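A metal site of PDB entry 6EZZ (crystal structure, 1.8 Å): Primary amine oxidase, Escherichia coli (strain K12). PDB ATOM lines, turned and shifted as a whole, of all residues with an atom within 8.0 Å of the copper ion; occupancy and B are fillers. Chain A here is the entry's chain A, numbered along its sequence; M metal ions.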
ATOM      1  N   VAL A 367     -28.343   6.652 -31.731  1.00  0.00           N
ATOM      2  CA  VAL A 367     -27.976   6.916 -30.347  1.00  0.00           C
ATOM      3  C   VAL A 367     -29.258   6.983 -29.520  1.00  0.00           C
ATOM      4  O   VAL A 367     -29.891   8.046 -29.462  1.00  0.00           O
ATOM      5  CB  VAL A 367     -27.200   8.213 -30.224  1.00  0.00           C
ATOM      6  CG1 VAL A 367     -26.747   8.445 -28.785  1.00  0.00           C
ATOM      7  CG2 VAL A 367     -25.982   8.157 -31.142  1.00  0.00           C
ATOM      8  N   TYR A 369     -31.719   6.462 -26.044  1.00  0.00           N
ATOM      9  CA  TYR A 369     -31.581   6.723 -24.609  1.00  0.00           C
ATOM     10  C   TYR A 369     -32.411   5.754 -23.749  1.00  0.00           C
ATOM     11  O   TYR A 369     -33.336   5.121 -24.241  1.00  0.00           O
ATOM     12  CB  TYR A 369     -31.880   8.191 -24.336  1.00  0.00           C
ATOM     13  CG  TYR A 369     -30.701   9.066 -24.747  1.00  0.00           C
ATOM     14  CD1 TYR A 369     -30.457   9.362 -26.080  1.00  0.00           C
ATOM     15  CD2 TYR A 369     -29.785   9.523 -23.782  1.00  0.00           C
ATOM     16  CE1 TYR A 369     -29.353  10.120 -26.459  1.00  0.00           C
ATOM     17  CE2 TYR A 369     -28.678  10.275 -24.148  1.00  0.00           C
ATOM     18  CZ  TYR A 369     -28.464  10.562 -25.486  1.00  0.00           C
ATOM     19  OH  TYR A 369     -27.344  11.319 -25.822  1.00  0.00           O
ATOM     20  N   ASN A 465     -25.182  17.840 -30.279  1.00  0.00           N
ATOM     21  CA  ASN A 465     -24.232  17.807 -29.173  1.00  0.00           C
ATOM     22  C   ASN A 465     -23.004  16.912 -29.377  1.00  0.00           C
ATOM     23  O   ASN A 465     -21.930  17.201 -28.835  1.00  0.00           O
ATOM     24  CB  ASN A 465     -24.941  17.415 -27.862  1.00  0.00           C
ATOM     25  CG  ASN A 465     -25.707  16.128 -27.968  1.00  0.00           C
ATOM     26  OD1 ASN A 465     -26.596  16.016 -28.802  1.00  0.00           O
ATOM     27  ND2 ASN A 465     -25.349  15.146 -27.168  1.00  0.00           N
ATOM     28  N   TYR A 466     -23.148  15.853 -30.172  1.00  0.00           N
ATOM     29  CA  TYR A 466     -22.065  14.872 -30.356  1.00  0.00           C
ATOM     30  C   TYR A 466     -21.335  15.042 -31.700  1.00  0.00           C
ATOM     31  O   TYR A 466     -21.945  15.442 -32.683  1.00  0.00           O
ATOM     32  CB  TYR A 466     -22.622  13.441 -30.249  1.00  0.00           C
ATOM     33  CG  TYR A 466     -22.697  12.813 -28.850  1.00  0.00           C
ATOM     34  CD1 TYR A 466     -21.589  12.758 -28.013  1.00  0.00           C
ATOM     35  CD2 TYR A 466     -23.866  12.199 -28.413  1.00  0.00           C
ATOM     36  CE1 TYR A 466     -21.630  12.136 -26.748  1.00  0.00           C
ATOM     37  CE2 TYR A 466     -23.913  11.570 -27.134  1.00  0.00           C
ATOM     38  CZ  TYR A 466     -22.784  11.548 -26.312  1.00  0.00           C
ATOM     39  OH  TYR A 466     -22.794  10.906 -25.084  1.00  0.00           O
ATOM     40  N   TYR A 468     -18.758  12.857 -34.279  1.00  0.00           N
ATOM     41  CA  TYR A 468     -18.372  11.516 -34.645  1.00  0.00           C
ATOM     42  C   TYR A 468     -17.256  11.543 -35.673  1.00  0.00           C
ATOM     43  O   TYR A 468     -17.312  12.306 -36.636  1.00  0.00           O
ATOM     44  CB  TYR A 468     -19.571  10.761 -35.228  1.00  0.00           C
ATOM     45  CG  TYR A 468     -20.649  10.605 -34.187  1.00  0.00           C
ATOM     46  CD1 TYR A 468     -20.465   9.732 -33.113  1.00  0.00           C
ATOM     47  CD2 TYR A 468     -21.819  11.371 -34.234  1.00  0.00           C
ATOM     48  CE1 TYR A 468     -21.402   9.619 -32.105  1.00  0.00           C
ATOM     49  CE2 TYR A 468     -22.785  11.240 -33.250  1.00  0.00           C
ATOM     50  CZ  TYR A 468     -22.572  10.369 -32.189  1.00  0.00           C
ATOM     51  OH  TYR A 468     -23.499  10.254 -31.192  1.00  0.00           O
ATOM     52  N   ALA A 486     -16.187   8.915 -30.861  1.00  0.00           N
ATOM     53  CA  ALA A 486     -17.238   9.840 -30.412  1.00  0.00           C
ATOM     54  C   ALA A 486     -16.649  10.822 -29.388  1.00  0.00           C
ATOM     55  O   ALA A 486     -15.884  10.405 -28.511  1.00  0.00           O
ATOM     56  CB  ALA A 486     -18.390   9.054 -29.789  1.00  0.00           C
ATOM     57  N   THR A 487     -16.934  12.110 -29.560  1.00  0.00           N
ATOM     58  CA  THR A 487     -16.542  13.149 -28.622  1.00  0.00           C
ATOM     59  C   THR A 487     -17.667  14.161 -28.648  1.00  0.00           C
ATOM     60  O   THR A 487     -18.748  13.902 -29.193  1.00  0.00           O
ATOM     61  CB  THR A 487     -15.122  13.718 -28.925  1.00  0.00           C
ATOM     62  OG1 THR A 487     -14.782  14.753 -27.994  1.00  0.00           O
ATOM     63  CG2 THR A 487     -15.004  14.265 -30.355  1.00  0.00           C
ATOM     64  N   ILE A 489     -20.395  16.844 -26.483  1.00  0.00           N
ATOM     65  CA  ILE A 489     -21.017  17.249 -25.223  1.00  0.00           C
ATOM     66  C   ILE A 489     -22.141  16.241 -24.918  1.00  0.00           C
ATOM     67  O   ILE A 489     -22.971  16.002 -25.742  1.00  0.00           O
ATOM     68  CB  ILE A 489     -21.637  18.666 -25.312  1.00  0.00           C
ATOM     69  CG1 ILE A 489     -20.677  19.704 -25.911  1.00  0.00           C
ATOM     70  CG2 ILE A 489     -22.107  19.111 -23.920  1.00  0.00           C
ATOM     71  CD1 ILE A 489     -19.332  19.857 -25.227  1.00  0.00           C
ATOM     72  N   GLU A 490     -22.154  15.634 -23.738  1.00  0.00           N
ATOM     73  CA  GLU A 490     -23.241  14.726 -23.380  1.00  0.00           C
ATOM     74  C   GLU A 490     -24.606  15.394 -23.257  1.00  0.00           C
ATOM     75  O   GLU A 490     -24.693  16.558 -22.930  1.00  0.00           O
ATOM     76  CB  GLU A 490     -22.876  13.987 -22.107  1.00  0.00           C
ATOM     77  CG  GLU A 490     -21.802  12.926 -22.419  1.00  0.00           C
ATOM     78  CD  GLU A 490     -21.215  12.283 -21.185  1.00  0.00           C
ATOM     79  OE1 GLU A 490     -21.738  12.528 -20.064  1.00  0.00           O
ATOM     80  OE2 GLU A 490     -20.218  11.536 -21.350  1.00  0.00           O
ATOM     81  N   ALA A 491     -25.651  14.627 -23.598  1.00  0.00           N
ATOM     82  CA  ALA A 491     -27.037  15.056 -23.368  1.00  0.00           C
ATOM     83  C   ALA A 491     -27.337  14.751 -21.920  1.00  0.00           C
ATOM     84  O   ALA A 491     -27.284  13.564 -21.535  1.00  0.00           O
ATOM     85  CB  ALA A 491     -27.999  14.312 -24.269  1.00  0.00           C
ATOM     86  N   THR A 522     -27.466  10.826 -18.797  1.00  0.00           N
ATOM     87  CA  THR A 522     -28.388   9.734 -19.008  1.00  0.00           C
ATOM     88  C   THR A 522     -27.763   8.610 -19.838  1.00  0.00           C
ATOM     89  O   THR A 522     -27.153   8.893 -20.879  1.00  0.00           O
ATOM     90  CB  THR A 522     -29.679  10.234 -19.667  1.00  0.00           C
ATOM     91  OG1 THR A 522     -30.245  11.299 -18.877  1.00  0.00           O
ATOM     92  CG2 THR A 522     -30.687   9.132 -19.848  1.00  0.00           C
ATOM     93  N   THR A 523     -27.960   7.371 -19.401  1.00  0.00           N
ATOM     94  CA  THR A 523     -27.411   6.180 -20.034  1.00  0.00           C
ATOM     95  C   THR A 523     -28.050   5.998 -21.403  1.00  0.00           C
ATOM     96  O   THR A 523     -29.236   6.300 -21.604  1.00  0.00           O
ATOM     97  CB  THR A 523     -27.540   4.935 -19.114  1.00  0.00           C
ATOM     98  OG1 THR A 523     -26.788   5.168 -17.924  1.00  0.00           O
ATOM     99  CG2 THR A 523     -26.971   3.680 -19.775  1.00  0.00           C
ATOM    100  N   HIS A 524     -27.235   5.577 -22.355  1.00  0.00           N
ATOM    101  CA  HIS A 524     -27.697   5.418 -23.750  1.00  0.00           C
ATOM    102  C   HIS A 524     -26.708   4.537 -24.469  1.00  0.00           C
ATOM    103  O   HIS A 524     -25.745   4.149 -23.873  1.00  0.00           O
ATOM    104  CB  HIS A 524     -27.780   6.776 -24.441  1.00  0.00           C
ATOM    105  CG  HIS A 524     -26.485   7.521 -24.371  1.00  0.00           C
ATOM    106  ND1 HIS A 524     -26.080   8.163 -23.223  1.00  0.00           N
ATOM    107  CD2 HIS A 524     -25.489   7.649 -25.277  1.00  0.00           C
ATOM    108  CE1 HIS A 524     -24.869   8.657 -23.421  1.00  0.00           C
ATOM    109  NE2 HIS A 524     -24.498   8.384 -24.668  1.00  0.00           N
ATOM    110  N   GLN A 525     -26.943   4.235 -25.763  1.00  0.00           N
ATOM    111  CA  GLN A 525     -25.976   3.481 -26.537  1.00  0.00           C
ATOM    112  C   GLN A 525     -25.497   4.330 -27.696  1.00  0.00           C
ATOM    113  O   GLN A 525     -26.199   5.261 -28.103  1.00  0.00           O
ATOM    114  CB  GLN A 525     -26.602   2.211 -27.071  1.00  0.00           C
ATOM    115  CG  GLN A 525     -26.976   1.221 -25.962  1.00  0.00           C
ATOM    116  CD  GLN A 525     -27.514  -0.043 -26.534  1.00  0.00           C
ATOM    117  OE1 GLN A 525     -28.688  -0.114 -26.930  1.00  0.00           O
ATOM    118  NE2 GLN A 525     -26.660  -1.039 -26.595  1.00  0.00           N
ATOM    119  N   HIS A 526     -24.305   4.022 -28.227  1.00  0.00           N
ATOM    120  CA  HIS A 526     -23.917   4.504 -29.580  1.00  0.00           C
ATOM    121  C   HIS A 526     -23.826   3.292 -30.477  1.00  0.00           C
ATOM    122  O   HIS A 526     -23.051   2.387 -30.182  1.00  0.00           O
ATOM    123  CB  HIS A 526     -22.553   5.238 -29.551  1.00  0.00           C
ATOM    124  CG  HIS A 526     -22.537   6.460 -28.694  1.00  0.00           C
ATOM    125  ND1 HIS A 526     -22.762   7.723 -29.185  1.00  0.00           N
ATOM    126  CD2 HIS A 526     -22.360   6.621 -27.358  1.00  0.00           C
ATOM    127  CE1 HIS A 526     -22.711   8.601 -28.187  1.00  0.00           C
ATOM    128  NE2 HIS A 526     -22.466   7.953 -27.073  1.00  0.00           N
ATOM    129  N   TYR A 528     -23.330   1.924 -34.448  1.00  0.00           N
ATOM    130  CA  TYR A 528     -22.945   2.265 -35.815  1.00  0.00           C
ATOM    131  C   TYR A 528     -23.145   1.043 -36.667  1.00  0.00           C
ATOM    132  O   TYR A 528     -22.890  -0.039 -36.213  1.00  0.00           O
ATOM    133  CB  TYR A 528     -21.448   2.638 -35.891  1.00  0.00           C
ATOM    134  CG  TYR A 528     -21.003   3.624 -34.853  1.00  0.00           C
ATOM    135  CD1 TYR A 528     -21.162   4.992 -35.043  1.00  0.00           C
ATOM    136  CD2 TYR A 528     -20.429   3.210 -33.677  1.00  0.00           C
ATOM    137  CE1 TYR A 528     -20.746   5.917 -34.098  1.00  0.00           C
ATOM    138  CE2 TYR A 528     -20.039   4.133 -32.698  1.00  0.00           C
ATOM    139  CZ  TYR A 528     -20.201   5.494 -32.928  1.00  0.00           C
ATOM    140  OH  TYR A 528     -19.817   6.452 -32.018  1.00  0.00           O
ATOM    141  N   HIS A 613     -15.246   2.125 -24.540  1.00  0.00           N
ATOM    142  CA  HIS A 613     -16.439   2.121 -23.696  1.00  0.00           C
ATOM    143  C   HIS A 613     -16.967   0.691 -23.602  1.00  0.00           C
ATOM    144  O   HIS A 613     -16.628  -0.184 -24.415  1.00  0.00           O
ATOM    145  CB  HIS A 613     -17.562   2.973 -24.318  1.00  0.00           C
ATOM    146  CG  HIS A 613     -17.611   4.417 -23.888  1.00  0.00           C
ATOM    147  ND1 HIS A 613     -17.104   4.890 -22.699  1.00  0.00           N
ATOM    148  CD2 HIS A 613     -18.243   5.459 -24.466  1.00  0.00           C
ATOM    149  CE1 HIS A 613     -17.367   6.183 -22.590  1.00  0.00           C
ATOM    150  NE2 HIS A 613     -18.042   6.551 -23.656  1.00  0.00           N
ATOM    151  N   THR A 687     -21.684   0.623 -28.382  1.00  0.00           N
ATOM    152  CA  THR A 687     -21.294   0.723 -27.002  1.00  0.00           C
ATOM    153  C   THR A 687     -22.509   1.038 -26.135  1.00  0.00           C
ATOM    154  O   THR A 687     -23.503   1.546 -26.619  1.00  0.00           O
ATOM    155  CB  THR A 687     -20.282   1.866 -26.806  1.00  0.00           C
ATOM    156  OG1 THR A 687     -20.882   3.109 -27.201  1.00  0.00           O
ATOM    157  CG2 THR A 687     -19.033   1.606 -27.644  1.00  0.00           C
ATOM    158  N   THR A 688     -22.409   0.740 -24.854  1.00  0.00           N
ATOM    159  CA  THR A 688     -23.339   1.199 -23.850  1.00  0.00           C
ATOM    160  C   THR A 688     -22.593   2.247 -23.024  1.00  0.00           C
ATOM    161  O   THR A 688     -21.624   1.940 -22.322  1.00  0.00           O
ATOM    162  CB  THR A 688     -23.797   0.033 -22.967  1.00  0.00           C
ATOM    163  OG1 THR A 688     -24.604  -0.847 -23.758  1.00  0.00           O
ATOM    164  CG2 THR A 688     -24.634   0.528 -21.807  1.00  0.00           C
ATOM    165  N   HIS A 689     -23.051   3.481 -23.113  1.00  0.00           N
ATOM    166  CA  HIS A 689     -22.357   4.585 -22.540  1.00  0.00           C
ATOM    167  C   HIS A 689     -22.981   4.910 -21.178  1.00  0.00           C
ATOM    168  O   HIS A 689     -24.033   5.520 -21.114  1.00  0.00           O
ATOM    169  CB  HIS A 689     -22.387   5.786 -23.491  1.00  0.00           C
ATOM    170  CG  HIS A 689     -21.619   6.979 -23.014  1.00  0.00           C
ATOM    171  ND1 HIS A 689     -21.535   8.144 -23.755  1.00  0.00           N
ATOM    172  CD2 HIS A 689     -20.839   7.168 -21.915  1.00  0.00           C
ATOM    173  CE1 HIS A 689     -20.802   9.021 -23.082  1.00  0.00           C
ATOM    174  NE2 HIS A 689     -20.369   8.456 -21.966  1.00  0.00           N
ATOM    175  N   VAL A 690     -22.288   4.496 -20.125  1.00  0.00           N
ATOM    176  CA  VAL A 690     -22.569   4.956 -18.757  1.00  0.00           C
ATOM    177  C   VAL A 690     -21.553   6.052 -18.441  1.00  0.00           C
ATOM    178  O   VAL A 690     -20.356   5.866 -18.544  1.00  0.00           O
ATOM    179  CB  VAL A 690     -22.466   3.793 -17.737  1.00  0.00           C
ATOM    180  CG1 VAL A 690     -22.733   4.275 -16.302  1.00  0.00           C
ATOM    181  CG2 VAL A 690     -23.445   2.706 -18.079  1.00  0.00           C
ATOM    182  N   ALA A 691     -22.061   7.206 -18.043  1.00  0.00           N
ATOM    183  CA  ALA A 691     -21.277   8.414 -17.924  1.00  0.00           C
ATOM    184  C   ALA A 691     -20.416   8.504 -16.663  1.00  0.00           C
ATOM    185  O   ALA A 691     -20.645   7.834 -15.679  1.00  0.00           O
ATOM    186  CB  ALA A 691     -22.210   9.617 -17.986  1.00  0.00           C
ATOM    187  N   GLU A 695     -15.968  12.989 -18.281  1.00  0.00           N
ATOM    188  CA  GLU A 695     -16.547  13.287 -19.614  1.00  0.00           C
ATOM    189  C   GLU A 695     -17.334  14.587 -19.668  1.00  0.00           C
ATOM    190  O   GLU A 695     -18.037  14.873 -20.675  1.00  0.00           O
ATOM    191  CB  GLU A 695     -17.415  12.088 -20.074  1.00  0.00           C
ATOM    192  CG  GLU A 695     -16.714  10.737 -20.137  1.00  0.00           C
ATOM    193  CD  GLU A 695     -17.607   9.516 -20.247  1.00  0.00           C
ATOM    194  OE1 GLU A 695     -18.879   9.568 -20.049  1.00  0.00           O
ATOM    195  OE2 GLU A 695     -17.003   8.457 -20.536  1.00  0.00           O
ATOM    196  N   MET A 699     -16.382  15.451 -23.650  1.00  0.00           N
ATOM    197  CA  MET A 699     -16.065  14.052 -23.572  1.00  0.00           C
ATOM    198  C   MET A 699     -14.810  13.707 -24.329  1.00  0.00           C
ATOM    199  O   MET A 699     -14.781  13.863 -25.549  1.00  0.00           O
ATOM    200  CB  MET A 699     -17.203  13.200 -24.157  1.00  0.00           C
ATOM    201  CG  MET A 699     -16.872  11.726 -24.002  1.00  0.00           C
ATOM    202  SD  MET A 699     -18.188  10.565 -24.445  1.00  0.00           S
ATOM    203  CE  MET A 699     -18.143  10.466 -26.231  1.00  0.00           C
ATOM    204  N   GLU A 702     -13.735   8.670 -27.435  1.00  0.00           N
ATOM    205  CA  GLU A 702     -13.781   7.218 -27.214  1.00  0.00           C
ATOM    206  C   GLU A 702     -13.889   6.506 -28.569  1.00  0.00           C
ATOM    207  O   GLU A 702     -14.601   6.982 -29.419  1.00  0.00           O
ATOM    208  CB  GLU A 702     -15.012   6.884 -26.385  1.00  0.00           C
ATOM    209  CG  GLU A 702     -15.048   7.595 -25.025  1.00  0.00           C
ATOM    210  CD  GLU A 702     -14.278   6.883 -23.929  1.00  0.00           C
ATOM    211  OE1 GLU A 702     -13.590   5.863 -24.227  1.00  0.00           O
ATOM    212  OE2 GLU A 702     -14.341   7.371 -22.754  1.00  0.00           O
HETATM  213 CU    CU M   1     -22.627   8.811 -25.304  1.00  0.00          CU
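ND1 of His 526 lies within hydrogen-bond range of OH of Tyr 468.
O of His 526 lies within hydrogen-bond range of N of Thr 687 (2.9 Å).
NE2 of His 689 sits close to OE2 of Glu 490, 3.1 Å away.
A ring nitrogen (NE2) of His 613 lies close to a ring nitrogen (NE2) of His 689 (3.4 Å).
A ring nitrogen (NE2) of His 689 sits at hydrogen-bond distance from the side-chain carboxylate (OE1) of Glu 695, 2.7 Å away.
A ring nitrogen (ND1) of His 524 sits at hydrogen-bond distance from the backbone carbonyl oxygen (O) of Thr 522.
Within 4 Å of the copper ion: Tyr 466, His 524, His 526 and His 689.
The copper ion is bound by a ring nitrogen (NE2) of His 526 (2.0 Å).
A ring nitrogen (ND1) of His 689 binds the copper ion, at 2.0 Å.
The copper ion is bound by NE2 of His 524.
The copper ion is bound by the side-chain hydroxyl (OH) of Tyr 466 (2.1 Å).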
